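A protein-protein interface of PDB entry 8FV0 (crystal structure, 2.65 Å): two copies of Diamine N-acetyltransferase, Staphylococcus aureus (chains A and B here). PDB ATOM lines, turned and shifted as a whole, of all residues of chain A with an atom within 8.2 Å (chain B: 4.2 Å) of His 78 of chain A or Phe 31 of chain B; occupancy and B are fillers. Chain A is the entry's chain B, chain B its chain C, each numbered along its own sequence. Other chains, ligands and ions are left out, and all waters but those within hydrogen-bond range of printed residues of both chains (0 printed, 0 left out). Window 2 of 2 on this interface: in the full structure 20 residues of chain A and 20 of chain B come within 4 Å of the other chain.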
ATOM      1  N   GLU A  73     -13.527 -20.313 -14.796  1.00  0.00           N
ATOM      2  CA  GLU A  73     -12.423 -19.655 -14.096  1.00  0.00           C
ATOM      3  C   GLU A  73     -12.114 -18.295 -14.720  1.00  0.00           C
ATOM      4  O   GLU A  73     -10.960 -17.879 -14.826  1.00  0.00           O
ATOM      5  CB  GLU A  73     -11.178 -20.544 -14.081  1.00  0.00           C
ATOM      6  CG  GLU A  73     -11.408 -21.915 -13.463  1.00  0.00           C
ATOM      7  CD  GLU A  73     -11.819 -21.850 -12.002  1.00  0.00           C
ATOM      8  OE1 GLU A  73     -11.605 -20.799 -11.361  1.00  0.00           O
ATOM      9  OE2 GLU A  73     -12.358 -22.856 -11.492  1.00  0.00           O
ATOM     10  N   ILE A  74     -13.168 -17.596 -15.135  1.00  0.00           N
ATOM     11  CA  ILE A  74     -13.013 -16.284 -15.756  1.00  0.00           C
ATOM     12  C   ILE A  74     -12.491 -15.320 -14.696  1.00  0.00           C
ATOM     13  O   ILE A  74     -13.206 -14.972 -13.753  1.00  0.00           O
ATOM     14  CB  ILE A  74     -14.333 -15.788 -16.357  1.00  0.00           C
ATOM     15  CG1 ILE A  74     -14.828 -16.764 -17.427  1.00  0.00           C
ATOM     16  CG2 ILE A  74     -14.151 -14.399 -16.950  1.00  0.00           C
ATOM     17  CD1 ILE A  74     -16.238 -16.488 -17.909  1.00  0.00           C
ATOM     18  N   ASN A  75     -11.241 -14.892 -14.845  1.00  0.00           N
ATOM     19  CA  ASN A  75     -10.643 -13.903 -13.963  1.00  0.00           C
ATOM     20  C   ASN A  75     -10.574 -12.562 -14.683  1.00  0.00           C
ATOM     21  O   ASN A  75     -10.006 -12.469 -15.778  1.00  0.00           O
ATOM     22  CB  ASN A  75      -9.246 -14.331 -13.518  1.00  0.00           C
ATOM     23  CG  ASN A  75      -8.659 -13.392 -12.490  1.00  0.00           C
ATOM     24  OD1 ASN A  75      -8.060 -12.374 -12.833  1.00  0.00           O
ATOM     25  ND2 ASN A  75      -8.840 -13.723 -11.218  1.00  0.00           N
ATOM     26  N   TYR A  76     -11.140 -11.530 -14.063  1.00  0.00           N
ATOM     27  CA  TYR A  76     -11.250 -10.214 -14.674  1.00  0.00           C
ATOM     28  C   TYR A  76     -10.127  -9.266 -14.274  1.00  0.00           C
ATOM     29  O   TYR A  76     -10.162  -8.093 -14.661  1.00  0.00           O
ATOM     30  CB  TYR A  76     -12.599  -9.581 -14.317  1.00  0.00           C
ATOM     31  CG  TYR A  76     -13.788 -10.323 -14.876  1.00  0.00           C
ATOM     32  CD1 TYR A  76     -14.238 -10.079 -16.167  1.00  0.00           C
ATOM     33  CD2 TYR A  76     -14.464 -11.265 -14.113  1.00  0.00           C
ATOM     34  CE1 TYR A  76     -15.329 -10.755 -16.683  1.00  0.00           C
ATOM     35  CE2 TYR A  76     -15.555 -11.944 -14.620  1.00  0.00           C
ATOM     36  CZ  TYR A  76     -15.983 -11.686 -15.904  1.00  0.00           C
ATOM     37  OH  TYR A  76     -17.069 -12.362 -16.409  1.00  0.00           O
ATOM     38  N   ILE A  77      -9.144  -9.736 -13.509  1.00  0.00           N
ATOM     39  CA  ILE A  77      -7.969  -8.937 -13.178  1.00  0.00           C
ATOM     40  C   ILE A  77      -6.853  -9.315 -14.146  1.00  0.00           C
ATOM     41  O   ILE A  77      -6.298  -8.459 -14.844  1.00  0.00           O
ATOM     42  CB  ILE A  77      -7.528  -9.148 -11.719  1.00  0.00           C
ATOM     43  CG1 ILE A  77      -8.645  -8.755 -10.750  1.00  0.00           C
ATOM     44  CG2 ILE A  77      -6.255  -8.355 -11.432  1.00  0.00           C
ATOM     45  CD1 ILE A  77      -8.995  -7.284 -10.762  1.00  0.00           C
ATOM     46  N   HIS A  78      -6.514 -10.605 -14.184  1.00  0.00           N
ATOM     47  CA  HIS A  78      -5.530 -11.110 -15.130  1.00  0.00           C
ATOM     48  C   HIS A  78      -6.105 -11.295 -16.526  1.00  0.00           C
ATOM     49  O   HIS A  78      -5.340 -11.521 -17.470  1.00  0.00           O
ATOM     50  CB  HIS A  78      -4.960 -12.438 -14.629  1.00  0.00           C
ATOM     51  CG  HIS A  78      -4.601 -12.429 -13.176  1.00  0.00           C
ATOM     52  ND1 HIS A  78      -3.743 -11.501 -12.627  1.00  0.00           N
ATOM     53  CD2 HIS A  78      -4.984 -13.234 -12.158  1.00  0.00           C
ATOM     54  CE1 HIS A  78      -3.612 -11.736 -11.334  1.00  0.00           C
ATOM     55  NE2 HIS A  78      -4.354 -12.781 -11.023  1.00  0.00           N
ATOM     56  N   ARG A  79      -7.427 -11.212 -16.674  1.00  0.00           N
ATOM     57  CA  ARG A  79      -8.092 -11.284 -17.972  1.00  0.00           C
ATOM     58  C   ARG A  79      -7.725 -12.573 -18.712  1.00  0.00           C
ATOM     59  O   ARG A  79      -7.126 -12.559 -19.789  1.00  0.00           O
ATOM     60  CB  ARG A  79      -7.762 -10.047 -18.818  1.00  0.00           C
ATOM     61  CG  ARG A  79      -8.280  -8.734 -18.243  1.00  0.00           C
ATOM     62  CD  ARG A  79      -8.071  -7.576 -19.214  1.00  0.00           C
ATOM     63  N   ASN A  80      -8.103 -13.698 -18.111  1.00  0.00           N
ATOM     64  CA  ASN A  80      -7.937 -14.996 -18.751  1.00  0.00           C
ATOM     65  C   ASN A  80      -9.011 -15.938 -18.223  1.00  0.00           C
ATOM     66  O   ASN A  80      -9.677 -15.658 -17.223  1.00  0.00           O
ATOM     67  CB  ASN A  80      -6.529 -15.564 -18.525  1.00  0.00           C
ATOM     68  CG  ASN A  80      -6.205 -15.789 -17.058  1.00  0.00           C
ATOM     69  OD1 ASN A  80      -7.050 -16.227 -16.279  1.00  0.00           O
ATOM     70  ND2 ASN A  80      -4.968 -15.488 -16.676  1.00  0.00           N
ATOM     71  N   CYS A  81      -9.177 -17.060 -18.916  1.00  0.00           N
ATOM     72  CA  CYS A  81     -10.194 -18.033 -18.545  1.00  0.00           C
ATOM     73  C   CYS A  81      -9.876 -19.366 -19.202  1.00  0.00           C
ATOM     74  O   CYS A  81      -9.263 -19.417 -20.272  1.00  0.00           O
ATOM     75  CB  CYS A  81     -11.590 -17.573 -18.969  1.00  0.00           C
ATOM     76  SG  CYS A  81     -11.834 -17.626 -20.759  1.00  0.00           S
ATOM     77  N   ASN A 113     -13.687  -9.512 -23.273  1.00  0.00           N
ATOM     78  CA  ASN A 113     -12.482  -8.682 -23.248  1.00  0.00           C
ATOM     79  C   ASN A 113     -11.330  -9.405 -22.554  1.00  0.00           C
ATOM     80  O   ASN A 113     -10.513  -8.794 -21.861  1.00  0.00           O
ATOM     81  CB  ASN A 113     -12.767  -7.333 -22.581  1.00  0.00           C
ATOM     82  CG  ASN A 113     -11.724  -6.280 -22.913  1.00  0.00           C
ATOM     83  OD1 ASN A 113     -10.780  -6.537 -23.661  1.00  0.00           O
ATOM     84  ND2 ASN A 113     -11.898  -5.082 -22.366  1.00  0.00           N
ATOM     85  N   MET A 114     -11.255 -10.720 -22.752  1.00  0.00           N
ATOM     86  CA  MET A 114     -10.191 -11.510 -22.152  1.00  0.00           C
ATOM     87  C   MET A 114      -8.865 -11.264 -22.866  1.00  0.00           C
ATOM     88  O   MET A 114      -8.822 -10.918 -24.048  1.00  0.00           O
ATOM     89  CB  MET A 114     -10.531 -12.999 -22.210  1.00  0.00           C
ATOM     90  CG  MET A 114     -11.699 -13.415 -21.334  1.00  0.00           C
ATOM     91  SD  MET A 114     -11.259 -13.607 -19.594  1.00  0.00           S
ATOM     92  CE  MET A 114     -11.532 -11.950 -18.968  1.00  0.00           C
ATOM     93  N   HIS A 115      -7.773 -11.459 -22.127  1.00  0.00           N
ATOM     94  CA  HIS A 115      -6.434 -11.268 -22.663  1.00  0.00           C
ATOM     95  C   HIS A 115      -5.749 -12.572 -23.045  1.00  0.00           C
ATOM     96  O   HIS A 115      -4.820 -12.551 -23.858  1.00  0.00           O
ATOM     97  CB  HIS A 115      -5.561 -10.530 -21.640  1.00  0.00           C
ATOM     98  CG  HIS A 115      -4.163 -10.275 -22.111  1.00  0.00           C
ATOM     99  ND1 HIS A 115      -3.841  -9.232 -22.950  1.00  0.00           N
ATOM    100  CD2 HIS A 115      -3.005 -10.931 -21.861  1.00  0.00           C
ATOM    101  CE1 HIS A 115      -2.543  -9.254 -23.196  1.00  0.00           C
ATOM    102  NE2 HIS A 115      -2.012 -10.275 -22.548  1.00  0.00           N
ATOM    103  N   LYS A 116      -6.188 -13.698 -22.489  1.00  0.00           N
ATOM    104  CA  LYS A 116      -5.557 -14.982 -22.757  1.00  0.00           C
ATOM    105  C   LYS A 116      -6.550 -16.087 -22.440  1.00  0.00           C
ATOM    106  O   LYS A 116      -7.344 -15.964 -21.507  1.00  0.00           O
ATOM    107  CB  LYS A 116      -4.280 -15.148 -21.926  1.00  0.00           C
ATOM    108  CG  LYS A 116      -3.571 -16.479 -22.116  1.00  0.00           C
ATOM    109  CD  LYS A 116      -2.348 -16.586 -21.210  1.00  0.00           C
ATOM    110  CE  LYS A 116      -1.616 -17.906 -21.417  1.00  0.00           C
ATOM    111  NZ  LYS A 116      -0.425 -18.038 -20.531  1.00  0.00           N
ATOM    112  N   ILE A 117      -6.507 -17.158 -23.224  1.00  0.00           N
ATOM    113  CA  ILE A 117      -7.334 -18.333 -22.988  1.00  0.00           C
ATOM    114  C   ILE A 117      -6.405 -19.526 -22.828  1.00  0.00           C
ATOM    115  O   ILE A 117      -5.352 -19.595 -23.466  1.00  0.00           O
ATOM    116  CB  ILE A 117      -8.341 -18.572 -24.129  1.00  0.00           C
ATOM    117  CG1 ILE A 117      -9.204 -17.328 -24.344  1.00  0.00           C
ATOM    118  CG2 ILE A 117      -9.219 -19.770 -23.814  1.00  0.00           C
ATOM    119  CD1 ILE A 117     -10.076 -17.395 -25.578  1.00  0.00           C
ATOM    120  N   TYR A 118      -6.789 -20.466 -21.970  1.00  0.00           N
ATOM    121  CA  TYR A 118      -5.974 -21.650 -21.741  1.00  0.00           C
ATOM    122  C   TYR A 118      -6.869 -22.864 -21.547  1.00  0.00           C
ATOM    123  O   TYR A 118      -8.081 -22.751 -21.348  1.00  0.00           O
ATOM    124  CB  TYR A 118      -5.040 -21.470 -20.534  1.00  0.00           C
ATOM    125  CG  TYR A 118      -5.749 -21.200 -19.229  1.00  0.00           C
ATOM    126  CD1 TYR A 118      -6.110 -19.910 -18.872  1.00  0.00           C
ATOM    127  CD2 TYR A 118      -6.045 -22.232 -18.349  1.00  0.00           C
ATOM    128  CE1 TYR A 118      -6.752 -19.653 -17.679  1.00  0.00           C
ATOM    129  CE2 TYR A 118      -6.686 -21.986 -17.151  1.00  0.00           C
ATOM    130  CZ  TYR A 118      -7.039 -20.693 -16.822  1.00  0.00           C
ATOM    131  OH  TYR A 118      -7.680 -20.431 -15.633  1.00  0.00           O
ATOM    132  N   MET B  27       1.969  -9.236  -1.870  1.00  0.00           N
ATOM    133  CA  MET B  27       0.922  -9.820  -2.700  1.00  0.00           C
ATOM    134  C   MET B  27       1.311  -9.854  -4.175  1.00  0.00           C
ATOM    135  O   MET B  27       0.989 -10.818  -4.879  1.00  0.00           O
ATOM    136  CB  MET B  27      -0.380  -9.034  -2.526  1.00  0.00           C
ATOM    137  CG  MET B  27      -0.968  -9.079  -1.122  1.00  0.00           C
ATOM    138  SD  MET B  27      -1.644 -10.691  -0.680  1.00  0.00           S
ATOM    139  CE  MET B  27      -0.285 -11.400   0.246  1.00  0.00           C
ATOM    140  N   SER B  28       1.996  -8.816  -4.658  1.00  0.00           N
ATOM    141  CA  SER B  28       2.302  -8.728  -6.082  1.00  0.00           C
ATOM    142  C   SER B  28       3.054  -9.960  -6.569  1.00  0.00           C
ATOM    143  O   SER B  28       2.750 -10.498  -7.641  1.00  0.00           O
ATOM    144  CB  SER B  28       3.107  -7.459  -6.363  1.00  0.00           C
ATOM    145  OG  SER B  28       3.444  -7.363  -7.735  1.00  0.00           O
ATOM    146  N   TYR B  29       4.040 -10.425  -5.799  1.00  0.00           N
ATOM    147  CA  TYR B  29       4.797 -11.600  -6.216  1.00  0.00           C
ATOM    148  C   TYR B  29       3.903 -12.828  -6.335  1.00  0.00           C
ATOM    149  O   TYR B  29       4.184 -13.724  -7.138  1.00  0.00           O
ATOM    150  CB  TYR B  29       5.944 -11.864  -5.241  1.00  0.00           C
ATOM    151  CG  TYR B  29       7.107 -10.911  -5.413  1.00  0.00           C
ATOM    152  CD1 TYR B  29       7.109  -9.669  -4.794  1.00  0.00           C
ATOM    153  CD2 TYR B  29       8.200 -11.252  -6.202  1.00  0.00           C
ATOM    154  CE1 TYR B  29       8.168  -8.793  -4.952  1.00  0.00           C
ATOM    155  CE2 TYR B  29       9.264 -10.382  -6.365  1.00  0.00           C
ATOM    156  CZ  TYR B  29       9.242  -9.154  -5.737  1.00  0.00           C
ATOM    157  OH  TYR B  29      10.294  -8.281  -5.894  1.00  0.00           O
ATOM    158  N   TRP B  30       2.823 -12.886  -5.554  1.00  0.00           N
ATOM    159  CA  TRP B  30       1.847 -13.963  -5.649  1.00  0.00           C
ATOM    160  C   TRP B  30       0.629 -13.569  -6.477  1.00  0.00           C
ATOM    161  O   TRP B  30      -0.399 -14.252  -6.424  1.00  0.00           O
ATOM    162  CB  TRP B  30       1.426 -14.413  -4.249  1.00  0.00           C
ATOM    163  CG  TRP B  30       2.455 -15.287  -3.607  1.00  0.00           C
ATOM    164  CD1 TRP B  30       3.378 -14.920  -2.673  1.00  0.00           C
ATOM    165  CD2 TRP B  30       2.681 -16.677  -3.872  1.00  0.00           C
ATOM    166  NE1 TRP B  30       4.160 -15.997  -2.333  1.00  0.00           N
ATOM    167  CE2 TRP B  30       3.753 -17.087  -3.055  1.00  0.00           C
ATOM    168  CE3 TRP B  30       2.080 -17.614  -4.718  1.00  0.00           C
ATOM    169  CZ2 TRP B  30       4.236 -18.394  -3.060  1.00  0.00           C
ATOM    170  CZ3 TRP B  30       2.558 -18.911  -4.719  1.00  0.00           C
ATOM    171  CH2 TRP B  30       3.626 -19.289  -3.896  1.00  0.00           C
ATOM    172  N   PHE B  31       0.728 -12.484  -7.240  1.00  0.00           N
ATOM    173  CA  PHE B  31      -0.288 -12.050  -8.192  1.00  0.00           C
ATOM    174  C   PHE B  31      -1.619 -11.712  -7.534  1.00  0.00           C
ATOM    175  O   PHE B  31      -2.637 -11.599  -8.229  1.00  0.00           O
ATOM    176  CB  PHE B  31      -0.506 -13.109  -9.282  1.00  0.00           C
ATOM    177  CG  PHE B  31       0.768 -13.690  -9.825  1.00  0.00           C
ATOM    178  CD1 PHE B  31       1.611 -12.926 -10.615  1.00  0.00           C
ATOM    179  CD2 PHE B  31       1.123 -15.000  -9.547  1.00  0.00           C
ATOM    180  CE1 PHE B  31       2.784 -13.457 -11.116  1.00  0.00           C
ATOM    181  CE2 PHE B  31       2.294 -15.536 -10.046  1.00  0.00           C
ATOM    182  CZ  PHE B  31       3.126 -14.763 -10.831  1.00  0.00           C
ATOM    183  N   GLU B  32      -1.642 -11.544  -6.216  1.00  0.00           N
ATOM    184  CA  GLU B  32      -2.857 -11.190  -5.502  1.00  0.00           C
ATOM    185  C   GLU B  32      -3.047  -9.674  -5.494  1.00  0.00           C
ATOM    186  O   GLU B  32      -2.169  -8.906  -5.891  1.00  0.00           O
ATOM    187  CB  GLU B  32      -2.813 -11.729  -4.071  1.00  0.00           C
ATOM    188  CG  GLU B  32      -2.736 -13.247  -3.966  1.00  0.00           C
ATOM    189  CD  GLU B  32      -4.061 -13.926  -4.256  1.00  0.00           C
ATOM    190  OE1 GLU B  32      -5.006 -13.234  -4.690  1.00  0.00           O
ATOM    191  OE2 GLU B  32      -4.159 -15.154  -4.043  1.00  0.00           O
ATOM    192  N   ASP B 122       6.357 -16.370 -10.178  1.00  0.00           N
ATOM    193  CA  ASP B 122       6.783 -15.397 -11.177  1.00  0.00           C
ATOM    194  C   ASP B 122       8.145 -15.789 -11.738  1.00  0.00           C
ATOM    195  O   ASP B 122       9.069 -16.120 -10.990  1.00  0.00           O
ATOM    196  CB  ASP B 122       6.841 -13.999 -10.564  1.00  0.00           C
ATOM    197  CG  ASP B 122       7.064 -12.916 -11.604  1.00  0.00           C
ATOM    198  OD1 ASP B 122       7.987 -13.058 -12.434  1.00  0.00           O
ATOM    199  OD2 ASP B 122       6.308 -11.922 -11.597  1.00  0.00           O
ATOM    200  N   GLN B 146       0.491 -14.825 -17.990  1.00  0.00           N
ATOM    201  CA  GLN B 146      -0.572 -15.496 -17.256  1.00  0.00           C
ATOM    202  C   GLN B 146      -1.180 -14.619 -16.172  1.00  0.00           C
ATOM    203  O   GLN B 146      -2.329 -14.854 -15.782  1.00  0.00           O
ATOM    204  CB  GLN B 146      -0.044 -16.791 -16.630  1.00  0.00           C
ATOM    205  CG  GLN B 146      -1.107 -17.633 -15.936  1.00  0.00           C
ATOM    206  CD  GLN B 146      -2.158 -18.156 -16.895  1.00  0.00           C
ATOM    207  OE1 GLN B 146      -1.957 -18.162 -18.108  1.00  0.00           O
ATOM    208  NE2 GLN B 146      -3.289 -18.594 -16.354  1.00  0.00           N
ATOM    209  N   PHE B 147      -0.450 -13.621 -15.678  1.00  0.00           N
ATOM    210  CA  PHE B 147      -0.973 -12.758 -14.627  1.00  0.00           C
ATOM    211  C   PHE B 147      -0.766 -11.301 -15.007  1.00  0.00           C
ATOM    212  O   PHE B 147      -0.107 -10.985 -15.996  1.00  0.00           O
ATOM    213  CB  PHE B 147      -0.308 -13.071 -13.280  1.00  0.00           C
ATOM    214  CG  PHE B 147      -0.493 -14.494 -12.835  1.00  0.00           C
ATOM    215  CD1 PHE B 147      -1.667 -14.892 -12.217  1.00  0.00           C
ATOM    216  CD2 PHE B 147       0.503 -15.434 -13.039  1.00  0.00           C
ATOM    217  CE1 PHE B 147      -1.842 -16.200 -11.808  1.00  0.00           C
ATOM    218  CE2 PHE B 147       0.334 -16.743 -12.632  1.00  0.00           C
ATOM    219  CZ  PHE B 147      -0.841 -17.127 -12.016  1.00  0.00           C
ATOM    220  N   TYR B 148      -1.347 -10.408 -14.208  1.00  0.00           N
ATOM    221  CA  TYR B 148      -1.208  -8.971 -14.422  1.00  0.00           C
ATOM    222  C   TYR B 148      -0.926  -8.305 -13.087  1.00  0.00           C
ATOM    223  O   TYR B 148      -1.752  -8.373 -12.173  1.00  0.00           O
ATOM    224  CB  TYR B 148      -2.467  -8.371 -15.059  1.00  0.00           C
ATOM    225  CG  TYR B 148      -2.345  -6.892 -15.342  1.00  0.00           C
ATOM    226  CD1 TYR B 148      -1.851  -6.439 -16.557  1.00  0.00           C
ATOM    227  CD2 TYR B 148      -2.713  -5.947 -14.392  1.00  0.00           C
ATOM    228  CE1 TYR B 148      -1.731  -5.088 -16.824  1.00  0.00           C
ATOM    229  CE2 TYR B 148      -2.598  -4.592 -14.649  1.00  0.00           C
ATOM    230  CZ  TYR B 148      -2.107  -4.170 -15.867  1.00  0.00           C
ATOM    231  OH  TYR B 148      -1.987  -2.826 -16.138  1.00  0.00           O
ATOM    232  N   TYR B 153       1.758  -7.432 -17.769  1.00  0.00           N
ATOM    233  CA  TYR B 153       1.469  -8.859 -17.807  1.00  0.00           C
ATOM    234  C   TYR B 153       2.747  -9.631 -17.510  1.00  0.00           C
ATOM    235  O   TYR B 153       3.810  -9.331 -18.061  1.00  0.00           O
ATOM    236  CB  TYR B 153       0.899  -9.266 -19.164  1.00  0.00           C
ATOM    237  CG  TYR B 153      -0.531  -8.828 -19.373  1.00  0.00           C
ATOM    238  CD1 TYR B 153      -1.587  -9.535 -18.808  1.00  0.00           C
ATOM    239  CD2 TYR B 153      -0.826  -7.708 -20.136  1.00  0.00           C
ATOM    240  CE1 TYR B 153      -2.897  -9.133 -18.999  1.00  0.00           C
ATOM    241  CE2 TYR B 153      -2.128  -7.301 -20.333  1.00  0.00           C
ATOM    242  CZ  TYR B 153      -3.160  -8.014 -19.764  1.00  0.00           C
ATOM    243  OH  TYR B 153      -4.457  -7.599 -19.966  1.00  0.00           O
ATOM    244  N   ALA B 156       4.699 -16.912 -15.728  1.00  0.00           N
ATOM    245  CA  ALA B 156       4.787 -17.671 -14.489  1.00  0.00           C
ATOM    246  C   ALA B 156       5.227 -19.094 -14.785  1.00  0.00           C
ATOM    247  O   ALA B 156       4.709 -19.731 -15.706  1.00  0.00           O
ATOM    248  CB  ALA B 156       3.439 -17.677 -13.755  1.00  0.00           C
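The backbone carbonyl oxygen (O) of Phe 31 of chain B sits close to a ring nitrogen (NE2) of His 78 of chain A (3.5 Å).
The side-chain amide nitrogen (ND2) of Asn 80 of chain A is in hydrogen-bond range of the backbone carbonyl oxygen (O) of Gln 146 of chain B.
The side-chain amide oxygen (OE1) of Gln 146 of chain B is in hydrogen-bond range of the side-chain amino group (NZ) of Lys 116 of chain A (2.9 Å).
ND1 of His 78 of chain A sits at hydrogen-bond distance from N of Tyr 148 of chain B (3.1 Å).
The side-chain hydroxyl (OH) of Tyr 153 of chain B lies close to a ring nitrogen (ND1) of His 115 of chain A (3.5 Å).
The backbone NH (N) of His 78 of chain A sits at hydrogen-bond distance from the side-chain amide oxygen (OD1) of Asn 75 of chain A (2.7 Å).
The backbone NH of Asn 75 of chain A lies within hydrogen-bond range of the backbone carbonyl oxygen of Asn 80 of chain A (2.9 Å).
The backbone carbonyl oxygen of Arg 79 of chain A lies within hydrogen-bond range of the backbone NH of Lys 116 of chain A.
The backbone NH (N) of Asn 80 of chain A sits at hydrogen-bond distance from the side-chain sulfur (SD) of Met 114 of chain A (3.5 Å).
O of Lys 116 of chain A sits at hydrogen-bond distance from N of Cys 81 of chain A, 3.4 Å away.
O of Cys 81 of chain A lies within hydrogen-bond range of N of Tyr 118 of chain A (3.2 Å).
No position is printed for both chains.
Of the 11 pairs that touch across the chains among the printed residues, none has its exchanged pair printed and touching as well.
Of the 15 printed residues of chain A, 7 touch a printed residue of chain B.
Hydrophobic or aromatic side chains of chain A within 4 Å of the printed part of chain B: His 78, His 115 and Tyr 118.
Hydrophobic or aromatic side chains of chain B within 4 Å of the printed part of chain A: Phe 31, Phe 147, Tyr 148 and Tyr 153.
Along chain B the printed residues that touch a printed residue of chain A span positions 31 to 153.
Among the printed residues, 11 pairs touch across the chains.
Among the printed residues, no Asp or Glu carboxylate lies within 4 Å of a Lys or Arg side-chain nitrogen of the other chain.
Of chain B, only Phe 31, Gln 146, Phe 147, Tyr 148 and Tyr 153 come within 4 Å of His 78 of chain A.
Printed residues of chain B within 4 Å of Asn 80 of chain A: Gln 146.
Of the printed residues of chain B, His 115 of chain A touches Tyr 153 (3.4 Å).
Trp 30 of chain B touches none of the printed residues of chain A.
Of chain A, only His 78 comes within 4 Å of Phe 31 of chain B.
Of the printed residues of chain A, Tyr 148 of chain B touches Ile 77 (3.8 Å) and His 78 (3.1 Å).
Of the printed residues of chain A, Tyr 153 of chain B touches His 78 (3.7 Å), Arg 79 (3.7 Å) and His 115 (3.4 Å).
The nearest printed residue of chain B that does not touch His 78 of chain A is Glu 32 of chain B (5.5 Å).
The nearest printed residue of chain B that does not touch Lys 116 of chain A is Phe 147 of chain B (6.6 Å).
Among the printed residues, merely in contact across the chains: His 78 of chain A with Phe 147 of chain B, Arg 79 of chain A with Tyr 153 of chain B, His 78 of chain A with Tyr 153 of chain B, His 78 of chain A with Gln 146 of chain B, Ile 77 of chain A with Tyr 148 of chain B and Tyr 118 of chain A with Gln 146 of chain B.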
